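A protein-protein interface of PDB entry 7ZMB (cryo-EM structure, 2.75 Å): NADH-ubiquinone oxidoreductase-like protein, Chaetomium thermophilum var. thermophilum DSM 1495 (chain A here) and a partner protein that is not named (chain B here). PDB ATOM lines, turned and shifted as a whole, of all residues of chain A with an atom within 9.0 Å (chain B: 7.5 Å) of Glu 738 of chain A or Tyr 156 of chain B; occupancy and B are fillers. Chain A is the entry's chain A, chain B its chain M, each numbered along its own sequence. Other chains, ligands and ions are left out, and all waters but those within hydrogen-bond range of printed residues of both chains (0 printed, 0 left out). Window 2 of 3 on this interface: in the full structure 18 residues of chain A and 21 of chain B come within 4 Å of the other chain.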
ATOM      1  N   ARG A 728      16.600  -1.869   7.353  1.00  0.00           N
ATOM      2  CA  ARG A 728      15.772  -0.896   6.666  1.00  0.00           C
ATOM      3  C   ARG A 728      14.475  -1.532   6.186  1.00  0.00           C
ATOM      4  O   ARG A 728      14.445  -2.695   5.779  1.00  0.00           O
ATOM      5  CB  ARG A 728      16.588  -0.293   5.524  1.00  0.00           C
ATOM      6  CG  ARG A 728      17.466   0.823   6.044  1.00  0.00           C
ATOM      7  CD  ARG A 728      18.659   1.211   5.176  1.00  0.00           C
ATOM      8  NE  ARG A 728      18.372   1.773   3.863  1.00  0.00           N
ATOM      9  CZ  ARG A 728      18.421   1.083   2.731  1.00  0.00           C
ATOM     10  NH1 ARG A 728      18.749  -0.199   2.745  1.00  0.00           N
ATOM     11  NH2 ARG A 728      18.161   1.677   1.579  1.00  0.00           N
ATOM     12  N   ASN A 730      12.455  -0.643   3.658  1.00  0.00           N
ATOM     13  CA  ASN A 730      12.305  -0.690   2.213  1.00  0.00           C
ATOM     14  C   ASN A 730      13.480  -1.393   1.540  1.00  0.00           C
ATOM     15  O   ASN A 730      13.888  -1.005   0.444  1.00  0.00           O
ATOM     16  CB  ASN A 730      12.138   0.728   1.663  1.00  0.00           C
ATOM     17  CG  ASN A 730      11.139   1.557   2.463  1.00  0.00           C
ATOM     18  OD1 ASN A 730      10.179   1.030   3.016  1.00  0.00           O
ATOM     19  ND2 ASN A 730      11.364   2.859   2.520  1.00  0.00           N
ATOM     20  N   GLY A 735       9.597   2.267  -1.923  1.00  0.00           N
ATOM     21  CA  GLY A 735       9.884   3.292  -0.936  1.00  0.00           C
ATOM     22  C   GLY A 735      11.121   4.073  -1.323  1.00  0.00           C
ATOM     23  O   GLY A 735      11.993   3.598  -2.048  1.00  0.00           O
ATOM     24  N   MET A 736      11.186   5.307  -0.844  1.00  0.00           N
ATOM     25  CA  MET A 736      12.362   6.141  -1.032  1.00  0.00           C
ATOM     26  C   MET A 736      13.397   5.829   0.032  1.00  0.00           C
ATOM     27  O   MET A 736      13.065   5.492   1.169  1.00  0.00           O
ATOM     28  CB  MET A 736      12.006   7.629  -0.979  1.00  0.00           C
ATOM     29  CG  MET A 736      11.327   8.162  -2.222  1.00  0.00           C
ATOM     30  SD  MET A 736      10.777   9.879  -2.061  1.00  0.00           S
ATOM     31  CE  MET A 736      10.174   9.899  -0.377  1.00  0.00           C
ATOM     32  N   GLU A 737      14.665   5.947  -0.354  1.00  0.00           N
ATOM     33  CA  GLU A 737      15.794   5.774   0.544  1.00  0.00           C
ATOM     34  C   GLU A 737      16.805   6.874   0.257  1.00  0.00           C
ATOM     35  O   GLU A 737      16.655   7.649  -0.692  1.00  0.00           O
ATOM     36  CB  GLU A 737      16.418   4.386   0.386  1.00  0.00           C
ATOM     37  CG  GLU A 737      15.518   3.253   0.826  1.00  0.00           C
ATOM     38  CD  GLU A 737      15.088   3.377   2.278  1.00  0.00           C
ATOM     39  OE1 GLU A 737      15.965   3.500   3.159  1.00  0.00           O
ATOM     40  OE2 GLU A 737      13.871   3.361   2.540  1.00  0.00           O
ATOM     41  N   GLU A 738      17.839   6.959   1.094  1.00  0.00           N
ATOM     42  CA  GLU A 738      18.898   7.931   0.848  1.00  0.00           C
ATOM     43  C   GLU A 738      19.695   7.565  -0.396  1.00  0.00           C
ATOM     44  O   GLU A 738      19.976   8.419  -1.245  1.00  0.00           O
ATOM     45  CB  GLU A 738      19.806   8.033   2.066  1.00  0.00           C
ATOM     46  CG  GLU A 738      21.135   8.686   1.793  1.00  0.00           C
ATOM     47  CD  GLU A 738      22.187   8.271   2.794  1.00  0.00           C
ATOM     48  OE1 GLU A 738      22.064   7.163   3.354  1.00  0.00           O
ATOM     49  OE2 GLU A 738      23.135   9.054   3.027  1.00  0.00           O
ATOM     50  N   ASP A 739      20.062   6.297  -0.522  1.00  0.00           N
ATOM     51  CA  ASP A 739      20.702   5.793  -1.725  1.00  0.00           C
ATOM     52  C   ASP A 739      19.708   5.482  -2.834  1.00  0.00           C
ATOM     53  O   ASP A 739      20.132   5.127  -3.938  1.00  0.00           O
ATOM     54  CB  ASP A 739      21.524   4.546  -1.391  1.00  0.00           C
ATOM     55  CG  ASP A 739      20.733   3.529  -0.604  1.00  0.00           C
ATOM     56  OD1 ASP A 739      19.617   3.864  -0.154  1.00  0.00           O
ATOM     57  OD2 ASP A 739      21.226   2.392  -0.434  1.00  0.00           O
ATOM     58  N   ARG A 740      18.409   5.602  -2.576  1.00  0.00           N
ATOM     59  CA  ARG A 740      17.373   5.410  -3.591  1.00  0.00           C
ATOM     60  C   ARG A 740      16.500   6.655  -3.599  1.00  0.00           C
ATOM     61  O   ARG A 740      15.407   6.669  -3.017  1.00  0.00           O
ATOM     62  CB  ARG A 740      16.556   4.144  -3.327  1.00  0.00           C
ATOM     63  CG  ARG A 740      16.157   3.401  -4.584  1.00  0.00           C
ATOM     64  CD  ARG A 740      15.465   2.073  -4.290  1.00  0.00           C
ATOM     65  NE  ARG A 740      14.397   2.184  -3.302  1.00  0.00           N
ATOM     66  CZ  ARG A 740      14.159   1.294  -2.342  1.00  0.00           C
ATOM     67  NH1 ARG A 740      14.909   0.211  -2.224  1.00  0.00           N
ATOM     68  NH2 ARG A 740      13.163   1.492  -1.497  1.00  0.00           N
ATOM     69  N   PRO A 741      16.970   7.737  -4.222  1.00  0.00           N
ATOM     70  CA  PRO A 741      16.143   8.952  -4.291  1.00  0.00           C
ATOM     71  C   PRO A 741      14.816   8.761  -5.000  1.00  0.00           C
ATOM     72  O   PRO A 741      13.820   9.373  -4.606  1.00  0.00           O
ATOM     73  CB  PRO A 741      17.055   9.938  -5.031  1.00  0.00           C
ATOM     74  CG  PRO A 741      18.426   9.453  -4.771  1.00  0.00           C
ATOM     75  CD  PRO A 741      18.324   7.966  -4.750  1.00  0.00           C
ATOM     76  N   MET A 742      14.766   7.918  -6.021  1.00  0.00           N
ATOM     77  CA  MET A 742      13.579   7.761  -6.849  1.00  0.00           C
ATOM     78  C   MET A 742      12.751   6.540  -6.485  1.00  0.00           C
ATOM     79  O   MET A 742      11.698   6.319  -7.091  1.00  0.00           O
ATOM     80  CB  MET A 742      13.993   7.681  -8.314  1.00  0.00           C
ATOM     81  CG  MET A 742      14.659   6.368  -8.657  1.00  0.00           C
ATOM     82  SD  MET A 742      16.268   6.252  -7.849  1.00  0.00           S
ATOM     83  CE  MET A 742      17.188   7.502  -8.743  1.00  0.00           C
ATOM     84  N   GLY A 743      13.191   5.746  -5.517  1.00  0.00           N
ATOM     85  CA  GLY A 743      12.401   4.599  -5.160  1.00  0.00           C
ATOM     86  C   GLY A 743      12.460   3.503  -6.209  1.00  0.00           C
ATOM     87  O   GLY A 743      13.361   3.437  -7.042  1.00  0.00           O
ATOM     88  N   TRP B 109      12.128  24.327   4.570  1.00  0.00           N
ATOM     89  CA  TRP B 109      13.120  24.225   5.664  1.00  0.00           C
ATOM     90  C   TRP B 109      12.532  24.797   6.944  1.00  0.00           C
ATOM     91  O   TRP B 109      11.775  25.771   6.859  1.00  0.00           O
ATOM     92  CB  TRP B 109      14.463  24.856   5.295  1.00  0.00           C
ATOM     93  CG  TRP B 109      15.186  24.113   4.219  1.00  0.00           C
ATOM     94  CD1 TRP B 109      15.048  24.280   2.874  1.00  0.00           C
ATOM     95  CD2 TRP B 109      16.166  23.078   4.399  1.00  0.00           C
ATOM     96  NE1 TRP B 109      15.877  23.423   2.205  1.00  0.00           N
ATOM     97  CE2 TRP B 109      16.576  22.673   3.112  1.00  0.00           C
ATOM     98  CE3 TRP B 109      16.741  22.463   5.515  1.00  0.00           C
ATOM     99  CZ2 TRP B 109      17.530  21.679   2.912  1.00  0.00           C
ATOM    100  CZ3 TRP B 109      17.679  21.478   5.314  1.00  0.00           C
ATOM    101  CH2 TRP B 109      18.067  21.092   4.032  1.00  0.00           C
ATOM    102  N   LYS B 135      15.544  12.695  11.819  1.00  0.00           N
ATOM    103  CA  LYS B 135      16.465  11.952  10.993  1.00  0.00           C
ATOM    104  C   LYS B 135      17.086  12.870   9.950  1.00  0.00           C
ATOM    105  O   LYS B 135      16.396  13.716   9.374  1.00  0.00           O
ATOM    106  CB  LYS B 135      15.762  10.796  10.303  1.00  0.00           C
ATOM    107  CG  LYS B 135      15.267   9.742  11.241  1.00  0.00           C
ATOM    108  CD  LYS B 135      15.222   8.416  10.532  1.00  0.00           C
ATOM    109  CE  LYS B 135      14.170   7.534  11.115  1.00  0.00           C
ATOM    110  NZ  LYS B 135      14.306   6.131  10.650  1.00  0.00           N
ATOM    111  N   PRO B 136      18.369  12.718   9.673  1.00  0.00           N
ATOM    112  CA  PRO B 136      18.962  13.452   8.557  1.00  0.00           C
ATOM    113  C   PRO B 136      18.433  12.917   7.239  1.00  0.00           C
ATOM    114  O   PRO B 136      19.110  12.179   6.523  1.00  0.00           O
ATOM    115  CB  PRO B 136      20.462  13.206   8.723  1.00  0.00           C
ATOM    116  CG  PRO B 136      20.579  12.015   9.582  1.00  0.00           C
ATOM    117  CD  PRO B 136      19.305  11.775  10.301  1.00  0.00           C
ATOM    118  N   GLU B 137      17.200  13.285   6.930  1.00  0.00           N
ATOM    119  CA  GLU B 137      16.500  12.822   5.747  1.00  0.00           C
ATOM    120  C   GLU B 137      15.331  13.764   5.529  1.00  0.00           C
ATOM    121  O   GLU B 137      14.836  14.375   6.474  1.00  0.00           O
ATOM    122  CB  GLU B 137      16.040  11.364   5.914  1.00  0.00           C
ATOM    123  CG  GLU B 137      15.154  10.811   4.815  1.00  0.00           C
ATOM    124  CD  GLU B 137      15.921  10.392   3.571  1.00  0.00           C
ATOM    125  OE1 GLU B 137      17.079  10.825   3.389  1.00  0.00           O
ATOM    126  OE2 GLU B 137      15.352   9.627   2.763  1.00  0.00           O
ATOM    127  N   GLU B 151      16.839  22.376   9.448  1.00  0.00           N
ATOM    128  CA  GLU B 151      18.065  23.094   9.124  1.00  0.00           C
ATOM    129  C   GLU B 151      19.295  22.468   9.768  1.00  0.00           C
ATOM    130  O   GLU B 151      20.413  22.710   9.308  1.00  0.00           O
ATOM    131  CB  GLU B 151      17.944  24.557   9.558  1.00  0.00           C
ATOM    132  CG  GLU B 151      17.230  25.457   8.583  1.00  0.00           C
ATOM    133  CD  GLU B 151      18.060  25.782   7.348  1.00  0.00           C
ATOM    134  OE1 GLU B 151      17.550  26.501   6.466  1.00  0.00           O
ATOM    135  OE2 GLU B 151      19.222  25.345   7.257  1.00  0.00           O
ATOM    136  N   HIS B 152      19.110  21.672  10.822  1.00  0.00           N
ATOM    137  CA  HIS B 152      20.221  20.984  11.462  1.00  0.00           C
ATOM    138  C   HIS B 152      20.870  19.958  10.546  1.00  0.00           C
ATOM    139  O   HIS B 152      21.994  19.529  10.815  1.00  0.00           O
ATOM    140  CB  HIS B 152      19.735  20.324  12.751  1.00  0.00           C
ATOM    141  CG  HIS B 152      20.752  19.440  13.401  1.00  0.00           C
ATOM    142  ND1 HIS B 152      20.783  18.076  13.210  1.00  0.00           N
ATOM    143  CD2 HIS B 152      21.779  19.726  14.234  1.00  0.00           C
ATOM    144  CE1 HIS B 152      21.783  17.560  13.898  1.00  0.00           C
ATOM    145  NE2 HIS B 152      22.403  18.540  14.531  1.00  0.00           N
ATOM    146  N   HIS B 153      20.206  19.624   9.442  1.00  0.00           N
ATOM    147  CA  HIS B 153      20.756  18.640   8.471  1.00  0.00           C
ATOM    148  C   HIS B 153      21.036  19.339   7.139  1.00  0.00           C
ATOM    149  O   HIS B 153      21.342  18.642   6.169  1.00  0.00           O
ATOM    150  CB  HIS B 153      19.798  17.450   8.291  1.00  0.00           C
ATOM    151  CG  HIS B 153      19.201  16.955   9.565  1.00  0.00           C
ATOM    152  ND1 HIS B 153      19.944  16.298  10.524  1.00  0.00           N
ATOM    153  CD2 HIS B 153      17.937  17.008  10.035  1.00  0.00           C
ATOM    154  CE1 HIS B 153      19.167  15.971  11.532  1.00  0.00           C
ATOM    155  NE2 HIS B 153      17.931  16.399  11.259  1.00  0.00           N
ATOM    156  N   ARG B 154      20.951  20.669   7.110  1.00  0.00           N
ATOM    157  CA  ARG B 154      21.181  21.402   5.870  1.00  0.00           C
ATOM    158  C   ARG B 154      22.551  21.085   5.288  1.00  0.00           C
ATOM    159  O   ARG B 154      22.688  20.888   4.077  1.00  0.00           O
ATOM    160  CB  ARG B 154      21.031  22.899   6.124  1.00  0.00           C
ATOM    161  CG  ARG B 154      21.776  23.777   5.154  1.00  0.00           C
ATOM    162  CD  ARG B 154      20.915  24.085   3.974  1.00  0.00           C
ATOM    163  NE  ARG B 154      19.710  24.778   4.388  1.00  0.00           N
ATOM    164  CZ  ARG B 154      18.874  25.372   3.557  1.00  0.00           C
ATOM    165  NH1 ARG B 154      19.110  25.357   2.257  1.00  0.00           N
ATOM    166  NH2 ARG B 154      17.800  25.978   4.029  1.00  0.00           N
ATOM    167  N   LYS B 155      23.572  21.003   6.141  1.00  0.00           N
ATOM    168  CA  LYS B 155      24.911  20.684   5.661  1.00  0.00           C
ATOM    169  C   LYS B 155      25.009  19.243   5.182  1.00  0.00           C
ATOM    170  O   LYS B 155      25.724  18.958   4.217  1.00  0.00           O
ATOM    171  CB  LYS B 155      25.943  20.957   6.756  1.00  0.00           C
ATOM    172  CG  LYS B 155      25.907  22.373   7.302  1.00  0.00           C
ATOM    173  CD  LYS B 155      27.284  22.824   7.751  1.00  0.00           C
ATOM    174  CE  LYS B 155      28.212  23.008   6.563  1.00  0.00           C
ATOM    175  NZ  LYS B 155      29.448  23.747   6.935  1.00  0.00           N
ATOM    176  N   TYR B 156      24.317  18.316   5.844  1.00  0.00           N
ATOM    177  CA  TYR B 156      24.393  16.921   5.419  1.00  0.00           C
ATOM    178  C   TYR B 156      23.629  16.689   4.124  1.00  0.00           C
ATOM    179  O   TYR B 156      24.093  15.958   3.244  1.00  0.00           O
ATOM    180  CB  TYR B 156      23.865  15.996   6.511  1.00  0.00           C
ATOM    181  CG  TYR B 156      23.882  14.548   6.082  1.00  0.00           C
ATOM    182  CD1 TYR B 156      25.066  13.836   6.034  1.00  0.00           C
ATOM    183  CD2 TYR B 156      22.719  13.903   5.699  1.00  0.00           C
ATOM    184  CE1 TYR B 156      25.089  12.524   5.631  1.00  0.00           C
ATOM    185  CE2 TYR B 156      22.733  12.601   5.289  1.00  0.00           C
ATOM    186  CZ  TYR B 156      23.917  11.911   5.260  1.00  0.00           C
ATOM    187  OH  TYR B 156      23.933  10.596   4.858  1.00  0.00           O
ATOM    188  N   LEU B 157      22.442  17.283   4.001  1.00  0.00           N
ATOM    189  CA  LEU B 157      21.630  17.062   2.814  1.00  0.00           C
ATOM    190  C   LEU B 157      22.241  17.736   1.595  1.00  0.00           C
ATOM    191  O   LEU B 157      22.168  17.200   0.485  1.00  0.00           O
ATOM    192  CB  LEU B 157      20.204  17.547   3.063  1.00  0.00           C
ATOM    193  CG  LEU B 157      19.434  16.723   4.096  1.00  0.00           C
ATOM    194  CD1 LEU B 157      17.943  16.843   3.931  1.00  0.00           C
ATOM    195  CD2 LEU B 157      19.851  15.264   4.007  1.00  0.00           C
ATOM    196  N   GLU B 158      22.864  18.901   1.775  1.00  0.00           N
ATOM    197  CA  GLU B 158      23.536  19.551   0.660  1.00  0.00           C
ATOM    198  C   GLU B 158      24.870  18.897   0.324  1.00  0.00           C
ATOM    199  O   GLU B 158      25.630  19.435  -0.486  1.00  0.00           O
ATOM    200  CB  GLU B 158      23.714  21.046   0.940  1.00  0.00           C
ATOM    201  CG  GLU B 158      24.860  21.420   1.862  1.00  0.00           C
ATOM    202  CD  GLU B 158      24.599  22.722   2.601  1.00  0.00           C
ATOM    203  OE1 GLU B 158      23.599  23.401   2.281  1.00  0.00           O
ATOM    204  OE2 GLU B 158      25.392  23.066   3.501  1.00  0.00           O
ATOM    205  N   SER B 159      25.155  17.743   0.921  1.00  0.00           N
ATOM    206  CA  SER B 159      26.314  16.936   0.586  1.00  0.00           C
ATOM    207  C   SER B 159      25.964  15.649  -0.142  1.00  0.00           C
ATOM    208  O   SER B 159      26.869  14.996  -0.672  1.00  0.00           O
ATOM    209  CB  SER B 159      27.096  16.581   1.855  1.00  0.00           C
ATOM    210  OG  SER B 159      27.958  15.486   1.618  1.00  0.00           O
ATOM    211  N   LEU B 160      24.693  15.266  -0.185  1.00  0.00           N
ATOM    212  CA  LEU B 160      24.332  13.986  -0.772  1.00  0.00           C
ATOM    213  C   LEU B 160      24.457  14.034  -2.293  1.00  0.00           C
ATOM    214  O   LEU B 160      24.097  15.037  -2.915  1.00  0.00           O
ATOM    215  CB  LEU B 160      22.911  13.599  -0.378  1.00  0.00           C
ATOM    216  CG  LEU B 160      22.645  13.363   1.100  1.00  0.00           C
ATOM    217  CD1 LEU B 160      21.168  13.114   1.327  1.00  0.00           C
ATOM    218  CD2 LEU B 160      23.487  12.210   1.600  1.00  0.00           C
ATOM    219  N   PRO B 161      24.949  12.962  -2.920  1.00  0.00           N
ATOM    220  CA  PRO B 161      25.078  12.962  -4.387  1.00  0.00           C
ATOM    221  C   PRO B 161      23.763  13.171  -5.106  1.00  0.00           C
ATOM    222  O   PRO B 161      23.737  13.797  -6.172  1.00  0.00           O
ATOM    223  CB  PRO B 161      25.669  11.576  -4.687  1.00  0.00           C
ATOM    224  CG  PRO B 161      26.254  11.111  -3.394  1.00  0.00           C
ATOM    225  CD  PRO B 161      25.396  11.694  -2.322  1.00  0.00           C
ATOM    226  N   GLN B 162      22.671  12.657  -4.560  1.00  0.00           N
ATOM    227  CA  GLN B 162      21.337  12.920  -5.068  1.00  0.00           C
ATOM    228  C   GLN B 162      20.396  13.006  -3.881  1.00  0.00           C
ATOM    229  O   GLN B 162      20.758  12.700  -2.745  1.00  0.00           O
ATOM    230  CB  GLN B 162      20.867  11.842  -6.050  1.00  0.00           C
ATOM    231  CG  GLN B 162      21.328  12.068  -7.483  1.00  0.00           C
ATOM    232  CD  GLN B 162      20.835  13.383  -8.054  1.00  0.00           C
ATOM    233  OE1 GLN B 162      19.719  13.820  -7.770  1.00  0.00           O
ATOM    234  NE2 GLN B 162      21.669  14.025  -8.862  1.00  0.00           N
ATOM    235  N   THR B 163      19.177  13.436  -4.157  1.00  0.00           N
ATOM    236  CA  THR B 163      18.157  13.539  -3.134  1.00  0.00           C
ATOM    237  C   THR B 163      16.812  13.313  -3.807  1.00  0.00           C
ATOM    238  O   THR B 163      16.733  13.056  -5.010  1.00  0.00           O
ATOM    239  CB  THR B 163      18.257  14.890  -2.417  1.00  0.00           C
ATOM    240  OG1 THR B 163      17.365  14.925  -1.301  1.00  0.00           O
ATOM    241  CG2 THR B 163      17.940  16.010  -3.366  1.00  0.00           C
ATOM    242  N   SER B 164      15.749  13.384  -3.018  1.00  0.00           N
ATOM    243  CA  SER B 164      14.414  13.151  -3.542  1.00  0.00           C
ATOM    244  C   SER B 164      13.712  14.427  -3.957  1.00  0.00           C
ATOM    245  O   SER B 164      12.930  14.410  -4.909  1.00  0.00           O
ATOM    246  CB  SER B 164      13.566  12.414  -2.505  1.00  0.00           C
ATOM    247  OG  SER B 164      13.695  13.025  -1.240  1.00  0.00           O
ATOM    248  N   LEU B 167      16.549  20.715  -2.912  1.00  0.00           N
ATOM    249  CA  LEU B 167      16.872  21.334  -1.636  1.00  0.00           C
ATOM    250  C   LEU B 167      16.692  22.841  -1.661  1.00  0.00           C
ATOM    251  O   LEU B 167      16.615  23.457  -0.596  1.00  0.00           O
ATOM    252  CB  LEU B 167      18.305  20.989  -1.232  1.00  0.00           C
ATOM    253  CG  LEU B 167      18.538  19.523  -0.864  1.00  0.00           C
ATOM    254  CD1 LEU B 167      19.878  19.366  -0.188  1.00  0.00           C
ATOM    255  CD2 LEU B 167      17.422  18.979   0.020  1.00  0.00           C
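The side-chain carboxylate of Glu 737 of chain A lies within salt-bridge range of the guanidinium group of Arg 728 of chain A (3.0 Å).
O of Met 736 of chain A is in hydrogen-bond range of ND2 of Asn 730 of chain A, at 3.4 Å.
The side-chain carboxylate (OE2) of Glu 737 of chain A sits at hydrogen-bond distance from the side-chain amide nitrogen (ND2) of Asn 730 of chain A, at 2.6 Å.
Hydrophobic or aromatic side chains of chain B that line the printed part of chain A: Tyr 156 and Leu 160.
Among the printed residues, no Asp or Glu carboxylate lies within 4 Å of a Lys or Arg side-chain nitrogen of the other chain.
OH of Tyr 156 of chain B is in hydrogen-bond range of OE2 of Glu 738 of chain A (2.5 Å).
Of the printed residues of chain B, Glu 738 of chain A touches Tyr 156 (2.5 Å) and Leu 160 (3.5 Å).
No residue of chain A comes within 4 Å of Ser 159 of chain B.
Of the printed residues of chain A, Glu 137 of chain B touches Glu 737.
Of the printed residues of chain B, Pro 741 of chain A touches Gln 162, Thr 163 and Ser 164.
The nearest residue of chain A that does not touch Tyr 156 of chain B is Asp 739 of chain A (7.9 Å).
Among the printed residues, merely in contact across the chains: Met 736 of chain A with Ser 164 of chain B (3.8 Å), Glu 737 of chain A with Glu 137 of chain B (3.996 Å), Glu 738 of chain A with Leu 160 of chain B (3.5 Å), Pro 741 of chain A with Gln 162 of chain B (3.6 Å), Pro 741 of chain A with Thr 163 of chain B (3.1 Å) and Pro 741 of chain A with Ser 164 of chain B (3.7 Å).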
